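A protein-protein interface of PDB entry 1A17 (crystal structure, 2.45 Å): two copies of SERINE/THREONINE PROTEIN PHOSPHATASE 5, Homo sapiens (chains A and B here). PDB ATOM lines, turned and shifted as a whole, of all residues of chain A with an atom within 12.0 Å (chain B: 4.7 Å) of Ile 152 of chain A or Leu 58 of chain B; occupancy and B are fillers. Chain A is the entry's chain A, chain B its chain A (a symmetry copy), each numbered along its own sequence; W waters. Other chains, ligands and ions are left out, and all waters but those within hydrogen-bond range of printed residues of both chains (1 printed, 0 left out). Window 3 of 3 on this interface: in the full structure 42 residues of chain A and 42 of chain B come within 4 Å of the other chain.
The backbone carbonyl oxygen of Thr 156 of chain A is in hydrogen-bond range of the guanidinium group of Arg 86 of chain B (2.8 Å).
The guanidinium group (NH2) of Arg 59 of chain B is in salt-bridge range of the side-chain carboxylate (OE2) of Glu 153 of chain A (3.3 Å).
O of Ile 152 of chain A sits close to NH1 of Arg 59 of chain B (2.3 Å).
O of Met 155 of chain A is in hydrogen-bond range of NH2 of Arg 59 of chain B.
The backbone carbonyl oxygen (O) of Arg 86 of chain B is in hydrogen-bond range of the side-chain hydroxyl (OG) of Ser 90 of chain B (2.7 Å).
Among the printed residues, pairs that only touch across the chains: Ile 152 of chain A with Leu 58 of chain B, Met 155 of chain A with Leu 55 of chain B, Met 155 of chain A with Ala 89 of chain B, Thr 156 of chain A with Leu 55 of chain B, Ile 157 of chain A with Leu 55 of chain B and Ile 157 of chain A with Arg 86 of chain B.
Of chain B, only Leu 58 (3.9 Å) and Arg 59 (2.3 Å) come within 4 Å of Ile 152 of chain A.
Leu 58 of chain B touches one residue of chain A.
No residue of chain A comes within 4 Å of Ser 54 of chain B.
Of chain A, only Met 155, Thr 156 and Ile 157 come within 4 Å of Leu 55 of chain B.
No residue of chain A comes within 4 Å of Ala 56 of chain B.
Arg 59 of chain B touches three residues of chain A.
Glu 61 of chain B touches none of the printed residues of chain A.
No residue of chain A comes within 4 Å of Ala 66 of chain B.
Ala 89 of chain B touches just one residue of chain A: Met 155.
Printed residues of chain B within 4 Å of Thr 156 of chain A: Leu 55 and Arg 86.
Printed residues of chain B within 4 Å of Met 155 of chain A: Leu 55 (3.6 Å), Arg 59 (3.1 Å) and Ala 89 (3.6 Å).
The nearest residue of chain A that does not touch Leu 58 of chain B is Met 155 of chain A (4.1 Å).
The nearest printed residue of chain B that does not touch Glu 153 of chain A is Leu 55 of chain B (6.5 Å).
Hydrophobic or aromatic side chains of chain B within 4 Å of the printed part of chain A: Leu 55 and Ala 89.
Hydrophobic or aromatic side chains of chain A within 4 Å of the printed part of chain B: Ile 152, Met 155 and Ile 157.
Along chain A the printed residues that touch a printed residue of chain B span positions 152 to 157.
Among the printed residues, 10 pairs touch across the chains.
Among the printed residues, Asp or Glu carboxylates within 4 Å of a Lys or Arg side-chain nitrogen of the other chain: Glu 153 of chain A with Arg 59 of chain B (3.3 Å).
No position is printed for both chains.
Of the 10 pairs that touch across the chains among the printed residues, none has its exchanged pair printed and touching as well.
Water W1 lies within hydrogen-bond range of the guanidinium group of Arg 86 of chain B and the side-chain sulfur of Met 155 of chain A.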
ATOM      1  N   LYS A 143       3.443  -7.509  -2.210  1.00  0.00           N
ATOM      2  CA  LYS A 143       4.546  -7.815  -1.312  1.00  0.00           C
ATOM      3  C   LYS A 143       4.051  -8.614  -0.132  1.00  0.00           C
ATOM      4  O   LYS A 143       4.692  -9.570   0.288  1.00  0.00           O
ATOM      5  CB  LYS A 143       5.224  -6.550  -0.795  1.00  0.00           C
ATOM      6  CG  LYS A 143       6.165  -6.858   0.356  1.00  0.00           C
ATOM      7  CD  LYS A 143       6.383  -5.684   1.285  1.00  0.00           C
ATOM      8  CE  LYS A 143       7.082  -6.142   2.568  1.00  0.00           C
ATOM      9  NZ  LYS A 143       7.830  -5.020   3.225  1.00  0.00           N
ATOM     10  N   ARG A 144       2.911  -8.207   0.407  1.00  0.00           N
ATOM     11  CA  ARG A 144       2.345  -8.892   1.550  1.00  0.00           C
ATOM     12  C   ARG A 144       2.125 -10.347   1.205  1.00  0.00           C
ATOM     13  O   ARG A 144       2.410 -11.237   2.004  1.00  0.00           O
ATOM     14  CB  ARG A 144       1.030  -8.241   2.000  1.00  0.00           C
ATOM     15  CG  ARG A 144       1.183  -6.857   2.609  1.00  0.00           C
ATOM     16  CD  ARG A 144      -0.179  -6.278   3.007  1.00  0.00           C
ATOM     17  NE  ARG A 144      -0.329  -4.881   2.584  1.00  0.00           N
ATOM     18  CZ  ARG A 144      -1.454  -4.360   2.100  1.00  0.00           C
ATOM     19  NH1 ARG A 144      -2.541  -5.113   1.986  1.00  0.00           N
ATOM     20  NH2 ARG A 144      -1.476  -3.101   1.681  1.00  0.00           N
ATOM     21  N   SER A 145       1.647 -10.597   0.002  1.00  0.00           N
ATOM     22  CA  SER A 145       1.414 -11.962  -0.411  1.00  0.00           C
ATOM     23  C   SER A 145       2.719 -12.753  -0.603  1.00  0.00           C
ATOM     24  O   SER A 145       2.743 -13.934  -0.279  1.00  0.00           O
ATOM     25  CB  SER A 145       0.539 -11.996  -1.664  1.00  0.00           C
ATOM     26  OG  SER A 145      -0.682 -11.299  -1.431  1.00  0.00           O
ATOM     27  N   VAL A 146       3.800 -12.131  -1.108  1.00  0.00           N
ATOM     28  CA  VAL A 146       5.077 -12.853  -1.295  1.00  0.00           C
ATOM     29  C   VAL A 146       5.642 -13.199   0.068  1.00  0.00           C
ATOM     30  O   VAL A 146       5.954 -14.346   0.358  1.00  0.00           O
ATOM     31  CB  VAL A 146       6.149 -12.034  -2.061  1.00  0.00           C
ATOM     32  CG1 VAL A 146       7.473 -12.761  -2.074  1.00  0.00           C
ATOM     33  CG2 VAL A 146       5.717 -11.818  -3.485  1.00  0.00           C
ATOM     34  N   VAL A 147       5.703 -12.206   0.930  1.00  0.00           N
ATOM     35  CA  VAL A 147       6.247 -12.395   2.251  1.00  0.00           C
ATOM     36  C   VAL A 147       5.500 -13.494   2.992  1.00  0.00           C
ATOM     37  O   VAL A 147       6.123 -14.398   3.545  1.00  0.00           O
ATOM     38  CB  VAL A 147       6.309 -11.050   2.972  1.00  0.00           C
ATOM     39  CG1 VAL A 147       6.930 -11.196   4.310  1.00  0.00           C
ATOM     40  CG2 VAL A 147       7.158 -10.096   2.134  1.00  0.00           C
ATOM     41  N   ASP A 148       4.177 -13.496   2.896  1.00  0.00           N
ATOM     42  CA  ASP A 148       3.365 -14.538   3.535  1.00  0.00           C
ATOM     43  C   ASP A 148       3.666 -15.935   2.966  1.00  0.00           C
ATOM     44  O   ASP A 148       3.507 -16.931   3.653  1.00  0.00           O
ATOM     45  CB  ASP A 148       1.867 -14.282   3.313  1.00  0.00           C
ATOM     46  CG  ASP A 148       1.284 -13.311   4.285  1.00  0.00           C
ATOM     47  OD1 ASP A 148       2.036 -12.631   5.019  1.00  0.00           O
ATOM     48  OD2 ASP A 148       0.044 -13.233   4.310  1.00  0.00           O
ATOM     49  N   SER A 149       4.062 -16.006   1.705  1.00  0.00           N
ATOM     50  CA  SER A 149       4.327 -17.286   1.061  1.00  0.00           C
ATOM     51  C   SER A 149       5.779 -17.747   1.101  1.00  0.00           C
ATOM     52  O   SER A 149       6.093 -18.831   0.597  1.00  0.00           O
ATOM     53  CB  SER A 149       3.865 -17.234  -0.408  1.00  0.00           C
ATOM     54  OG  SER A 149       2.468 -16.947  -0.534  1.00  0.00           O
ATOM     55  N   LEU A 150       6.660 -16.931   1.680  1.00  0.00           N
ATOM     56  CA  LEU A 150       8.084 -17.267   1.747  1.00  0.00           C
ATOM     57  C   LEU A 150       8.354 -18.552   2.527  1.00  0.00           C
ATOM     58  O   LEU A 150       8.004 -18.668   3.703  1.00  0.00           O
ATOM     59  CB  LEU A 150       8.895 -16.107   2.346  1.00  0.00           C
ATOM     60  CG  LEU A 150       9.137 -14.794   1.581  1.00  0.00           C
ATOM     61  CD1 LEU A 150       9.812 -13.819   2.517  1.00  0.00           C
ATOM     62  CD2 LEU A 150       9.993 -14.999   0.343  1.00  0.00           C
ATOM     63  N   ASP A 151       9.017 -19.502   1.880  1.00  0.00           N
ATOM     64  CA  ASP A 151       9.324 -20.774   2.514  1.00  0.00           C
ATOM     65  C   ASP A 151      10.560 -20.707   3.403  1.00  0.00           C
ATOM     66  O   ASP A 151      11.661 -21.113   3.029  1.00  0.00           O
ATOM     67  CB  ASP A 151       9.467 -21.876   1.466  1.00  0.00           C
ATOM     68  CG  ASP A 151       9.522 -23.269   2.084  1.00  0.00           C
ATOM     69  OD1 ASP A 151       8.831 -23.533   3.101  1.00  0.00           O
ATOM     70  OD2 ASP A 151      10.265 -24.102   1.532  1.00  0.00           O
ATOM     71  N   ILE A 152      10.353 -20.159   4.587  1.00  0.00           N
ATOM     72  CA  ILE A 152      11.403 -20.044   5.574  1.00  0.00           C
ATOM     73  C   ILE A 152      11.566 -21.399   6.254  1.00  0.00           C
ATOM     74  O   ILE A 152      12.674 -21.889   6.386  1.00  0.00           O
ATOM     75  CB  ILE A 152      11.089 -18.888   6.531  1.00  0.00           C
ATOM     76  CG1 ILE A 152      11.275 -17.571   5.757  1.00  0.00           C
ATOM     77  CG2 ILE A 152      11.960 -18.967   7.759  1.00  0.00           C
ATOM     78  CD1 ILE A 152      10.534 -16.393   6.315  1.00  0.00           C
ATOM     79  N   GLU A 153      10.449 -22.080   6.484  1.00  0.00           N
ATOM     80  CA  GLU A 153      10.443 -23.407   7.110  1.00  0.00           C
ATOM     81  C   GLU A 153      11.367 -24.470   6.494  1.00  0.00           C
ATOM     82  O   GLU A 153      11.877 -25.320   7.198  1.00  0.00           O
ATOM     83  CB  GLU A 153       9.007 -23.938   7.187  1.00  0.00           C
ATOM     84  CG  GLU A 153       8.809 -25.024   8.239  1.00  0.00           C
ATOM     85  CD  GLU A 153       9.425 -24.657   9.601  1.00  0.00           C
ATOM     86  OE1 GLU A 153       8.865 -23.758  10.275  1.00  0.00           O
ATOM     87  OE2 GLU A 153      10.473 -25.254   9.983  1.00  0.00           O
ATOM     88  N   SER A 154      11.573 -24.437   5.188  1.00  0.00           N
ATOM     89  CA  SER A 154      12.439 -25.418   4.549  1.00  0.00           C
ATOM     90  C   SER A 154      13.880 -24.989   4.562  1.00  0.00           C
ATOM     91  O   SER A 154      14.739 -25.687   4.019  1.00  0.00           O
ATOM     92  CB  SER A 154      12.034 -25.683   3.096  1.00  0.00           C
ATOM     93  OG  SER A 154      10.784 -26.354   3.005  1.00  0.00           O
ATOM     94  N   MET A 155      14.146 -23.797   5.079  1.00  0.00           N
ATOM     95  CA  MET A 155      15.524 -23.341   5.143  1.00  0.00           C
ATOM     96  C   MET A 155      16.202 -24.150   6.241  1.00  0.00           C
ATOM     97  O   MET A 155      15.530 -24.615   7.166  1.00  0.00           O
ATOM     98  CB  MET A 155      15.579 -21.844   5.425  1.00  0.00           C
ATOM     99  CG  MET A 155      15.024 -21.048   4.276  1.00  0.00           C
ATOM    100  SD  MET A 155      15.078 -19.259   4.405  1.00  0.00           S
ATOM    101  CE  MET A 155      14.356 -18.870   2.788  1.00  0.00           C
ATOM    102  N   THR A 156      17.515 -24.335   6.134  1.00  0.00           N
ATOM    103  CA  THR A 156      18.261 -25.115   7.123  1.00  0.00           C
ATOM    104  C   THR A 156      19.477 -24.468   7.749  1.00  0.00           C
ATOM    105  O   THR A 156      20.294 -23.800   7.103  1.00  0.00           O
ATOM    106  CB  THR A 156      18.724 -26.466   6.579  1.00  0.00           C
ATOM    107  OG1 THR A 156      19.339 -26.273   5.304  1.00  0.00           O
ATOM    108  CG2 THR A 156      17.552 -27.427   6.464  1.00  0.00           C
ATOM    109  N   ILE A 157      19.595 -24.738   9.038  1.00  0.00           N
ATOM    110  CA  ILE A 157      20.684 -24.253   9.850  1.00  0.00           C
ATOM    111  C   ILE A 157      21.872 -25.065   9.363  1.00  0.00           C
ATOM    112  O   ILE A 157      21.707 -26.147   8.774  1.00  0.00           O
ATOM    113  CB  ILE A 157      20.329 -24.481  11.346  1.00  0.00           C
ATOM    114  CG1 ILE A 157      20.740 -23.267  12.154  1.00  0.00           C
ATOM    115  CG2 ILE A 157      20.821 -25.838  11.879  1.00  0.00           C
ATOM    116  CD1 ILE A 157      19.936 -22.041  11.814  1.00  0.00           C
ATOM    117  N   GLU A 158      23.064 -24.513   9.486  1.00  0.00           N
ATOM    118  CA  GLU A 158      24.206 -25.269   9.021  1.00  0.00           C
ATOM    119  C   GLU A 158      24.427 -26.476   9.925  1.00  0.00           C
ATOM    120  O   GLU A 158      24.884 -26.329  11.055  1.00  0.00           O
ATOM    121  CB  GLU A 158      25.469 -24.406   8.967  1.00  0.00           C
ATOM    122  CG  GLU A 158      26.665 -25.112   8.316  1.00  0.00           C
ATOM    123  CD  GLU A 158      26.428 -25.460   6.850  1.00  0.00           C
ATOM    124  OE1 GLU A 158      26.749 -24.605   5.995  1.00  0.00           O
ATOM    125  OE2 GLU A 158      25.918 -26.578   6.559  1.00  0.00           O
ATOM    126  N   SER B  54      20.966 -15.682  11.707  1.00  0.00           N
ATOM    127  CA  SER B  54      20.170 -14.959  10.731  1.00  0.00           C
ATOM    128  C   SER B  54      18.914 -15.771  10.498  1.00  0.00           C
ATOM    129  O   SER B  54      17.815 -15.254  10.628  1.00  0.00           O
ATOM    130  CB  SER B  54      20.936 -14.792   9.409  1.00  0.00           C
ATOM    131  OG  SER B  54      20.102 -14.281   8.384  1.00  0.00           O
ATOM    132  N   LEU B  55      19.074 -17.065  10.239  1.00  0.00           N
ATOM    133  CA  LEU B  55      17.922 -17.911   9.972  1.00  0.00           C
ATOM    134  C   LEU B  55      17.014 -17.924  11.153  1.00  0.00           C
ATOM    135  O   LEU B  55      15.797 -17.861  11.002  1.00  0.00           O
ATOM    136  CB  LEU B  55      18.319 -19.339   9.594  1.00  0.00           C
ATOM    137  CG  LEU B  55      17.095 -20.245   9.344  1.00  0.00           C
ATOM    138  CD1 LEU B  55      16.181 -19.659   8.286  1.00  0.00           C
ATOM    139  CD2 LEU B  55      17.521 -21.642   8.946  1.00  0.00           C
ATOM    140  N   ALA B  56      17.593 -18.023  12.340  1.00  0.00           N
ATOM    141  CA  ALA B  56      16.774 -17.994  13.549  1.00  0.00           C
ATOM    142  C   ALA B  56      15.989 -16.696  13.571  1.00  0.00           C
ATOM    143  O   ALA B  56      14.908 -16.652  14.117  1.00  0.00           O
ATOM    144  CB  ALA B  56      17.628 -18.098  14.798  1.00  0.00           C
ATOM    145  N   TYR B  57      16.545 -15.625  13.011  1.00  0.00           N
ATOM    146  CA  TYR B  57      15.842 -14.346  12.978  1.00  0.00           C
ATOM    147  C   TYR B  57      14.762 -14.343  11.901  1.00  0.00           C
ATOM    148  O   TYR B  57      13.737 -13.687  12.060  1.00  0.00           O
ATOM    149  CB  TYR B  57      16.810 -13.186  12.761  1.00  0.00           C
ATOM    150  CG  TYR B  57      17.430 -12.635  14.044  1.00  0.00           C
ATOM    151  CD1 TYR B  57      16.651 -12.330  15.139  1.00  0.00           C
ATOM    152  CD2 TYR B  57      18.812 -12.446  14.151  1.00  0.00           C
ATOM    153  CE1 TYR B  57      17.210 -11.861  16.314  1.00  0.00           C
ATOM    154  CE2 TYR B  57      19.375 -11.981  15.306  1.00  0.00           C
ATOM    155  CZ  TYR B  57      18.566 -11.693  16.387  1.00  0.00           C
ATOM    156  OH  TYR B  57      19.128 -11.215  17.532  1.00  0.00           O
ATOM    157  N   LEU B  58      14.976 -15.060  10.798  1.00  0.00           N
ATOM    158  CA  LEU B  58      13.952 -15.118   9.747  1.00  0.00           C
ATOM    159  C   LEU B  58      12.732 -15.886  10.265  1.00  0.00           C
ATOM    160  O   LEU B  58      11.591 -15.489   9.995  1.00  0.00           O
ATOM    161  CB  LEU B  58      14.486 -15.785   8.476  1.00  0.00           C
ATOM    162  CG  LEU B  58      15.623 -15.106   7.713  1.00  0.00           C
ATOM    163  CD1 LEU B  58      16.153 -16.002   6.606  1.00  0.00           C
ATOM    164  CD2 LEU B  58      15.126 -13.802   7.152  1.00  0.00           C
ATOM    165  N   ARG B  59      12.979 -16.963  11.028  1.00  0.00           N
ATOM    166  CA  ARG B  59      11.906 -17.785  11.609  1.00  0.00           C
ATOM    167  C   ARG B  59      10.992 -17.044  12.610  1.00  0.00           C
ATOM    168  O   ARG B  59       9.835 -17.431  12.787  1.00  0.00           O
ATOM    169  CB  ARG B  59      12.453 -19.071  12.266  1.00  0.00           C
ATOM    170  CG  ARG B  59      13.077 -20.143  11.312  1.00  0.00           C
ATOM    171  CD  ARG B  59      12.045 -21.094  10.621  1.00  0.00           C
ATOM    172  NE  ARG B  59      12.505 -22.495  10.533  1.00  0.00           N
ATOM    173  CZ  ARG B  59      13.223 -22.988   9.528  1.00  0.00           C
ATOM    174  NH1 ARG B  59      13.561 -22.204   8.526  1.00  0.00           N
ATOM    175  NH2 ARG B  59      13.623 -24.252   9.524  1.00  0.00           N
ATOM    176  N   THR B  60      11.503 -16.015  13.288  1.00  0.00           N
ATOM    177  CA  THR B  60      10.694 -15.229  14.233  1.00  0.00           C
ATOM    178  C   THR B  60      10.298 -13.863  13.637  1.00  0.00           C
ATOM    179  O   THR B  60       9.975 -12.933  14.378  1.00  0.00           O
ATOM    180  CB  THR B  60      11.415 -15.030  15.631  1.00  0.00           C
ATOM    181  OG1 THR B  60      12.783 -14.645  15.447  1.00  0.00           O
ATOM    182  CG2 THR B  60      11.397 -16.309  16.435  1.00  0.00           C
ATOM    183  N   GLU B  61      10.366 -13.751  12.305  1.00  0.00           N
ATOM    184  CA  GLU B  61      10.011 -12.545  11.546  1.00  0.00           C
ATOM    185  C   GLU B  61      10.772 -11.232  11.815  1.00  0.00           C
ATOM    186  O   GLU B  61      10.260 -10.146  11.536  1.00  0.00           O
ATOM    187  CB  GLU B  61       8.500 -12.294  11.604  1.00  0.00           C
ATOM    188  CG  GLU B  61       7.676 -13.408  10.963  1.00  0.00           C
ATOM    189  CD  GLU B  61       6.164 -13.295  11.211  1.00  0.00           C
ATOM    190  OE1 GLU B  61       5.711 -12.364  11.914  1.00  0.00           O
ATOM    191  OE2 GLU B  61       5.417 -14.168  10.707  1.00  0.00           O
ATOM    192  N   TYR B  63      13.091  -9.381  10.313  1.00  0.00           N
ATOM    193  CA  TYR B  63      13.816  -9.197   9.068  1.00  0.00           C
ATOM    194  C   TYR B  63      15.012  -8.223   9.065  1.00  0.00           C
ATOM    195  O   TYR B  63      15.937  -8.406   8.297  1.00  0.00           O
ATOM    196  CB  TYR B  63      12.809  -8.920   7.951  1.00  0.00           C
ATOM    197  CG  TYR B  63      11.633  -9.909   7.899  1.00  0.00           C
ATOM    198  CD1 TYR B  63      11.848 -11.297   7.832  1.00  0.00           C
ATOM    199  CD2 TYR B  63      10.306  -9.454   7.905  1.00  0.00           C
ATOM    200  CE1 TYR B  63      10.782 -12.198   7.775  1.00  0.00           C
ATOM    201  CE2 TYR B  63       9.223 -10.362   7.850  1.00  0.00           C
ATOM    202  CZ  TYR B  63       9.474 -11.725   7.788  1.00  0.00           C
ATOM    203  OH  TYR B  63       8.424 -12.615   7.750  1.00  0.00           O
ATOM    204  N   ALA B  66      17.951 -10.254  10.786  1.00  0.00           N
ATOM    205  CA  ALA B  66      18.392 -11.317   9.857  1.00  0.00           C
ATOM    206  C   ALA B  66      19.258 -10.805   8.709  1.00  0.00           C
ATOM    207  O   ALA B  66      20.175 -11.484   8.257  1.00  0.00           O
ATOM    208  CB  ALA B  66      17.208 -12.027   9.296  1.00  0.00           C
ATOM    209  N   ARG B  86      20.624 -16.345   2.992  1.00  0.00           N
ATOM    210  CA  ARG B  86      20.089 -15.647   4.161  1.00  0.00           C
ATOM    211  C   ARG B  86      19.831 -14.182   3.777  1.00  0.00           C
ATOM    212  O   ARG B  86      18.790 -13.625   4.104  1.00  0.00           O
ATOM    213  CB  ARG B  86      21.100 -15.683   5.303  1.00  0.00           C
ATOM    214  CG  ARG B  86      21.479 -17.070   5.728  1.00  0.00           C
ATOM    215  CD  ARG B  86      20.281 -17.842   6.268  1.00  0.00           C
ATOM    216  NE  ARG B  86      20.766 -18.970   7.060  1.00  0.00           N
ATOM    217  CZ  ARG B  86      20.609 -20.244   6.734  1.00  0.00           C
ATOM    218  NH1 ARG B  86      19.955 -20.581   5.626  1.00  0.00           N
ATOM    219  NH2 ARG B  86      21.151 -21.183   7.496  1.00  0.00           N
ATOM    220  N   ALA B  89      16.890 -14.099   1.292  1.00  0.00           N
ATOM    221  CA  ALA B  89      15.651 -14.310   2.055  1.00  0.00           C
ATOM    222  C   ALA B  89      15.214 -13.094   2.882  1.00  0.00           C
ATOM    223  O   ALA B  89      14.029 -12.803   2.968  1.00  0.00           O
ATOM    224  CB  ALA B  89      15.778 -15.524   2.950  1.00  0.00           C
ATOM    225  N   SER B  90      16.158 -12.388   3.490  1.00  0.00           N
ATOM    226  CA  SER B  90      15.856 -11.206   4.304  1.00  0.00           C
ATOM    227  C   SER B  90      15.332 -10.063   3.458  1.00  0.00           C
ATOM    228  O   SER B  90      14.438  -9.340   3.879  1.00  0.00           O
ATOM    229  CB  SER B  90      17.113 -10.737   5.038  1.00  0.00           C
ATOM    230  OG  SER B  90      17.717 -11.806   5.748  1.00  0.00           O
HETATM  231  O   HOH W   1      18.551 -18.735   3.767  1.00  0.00           O
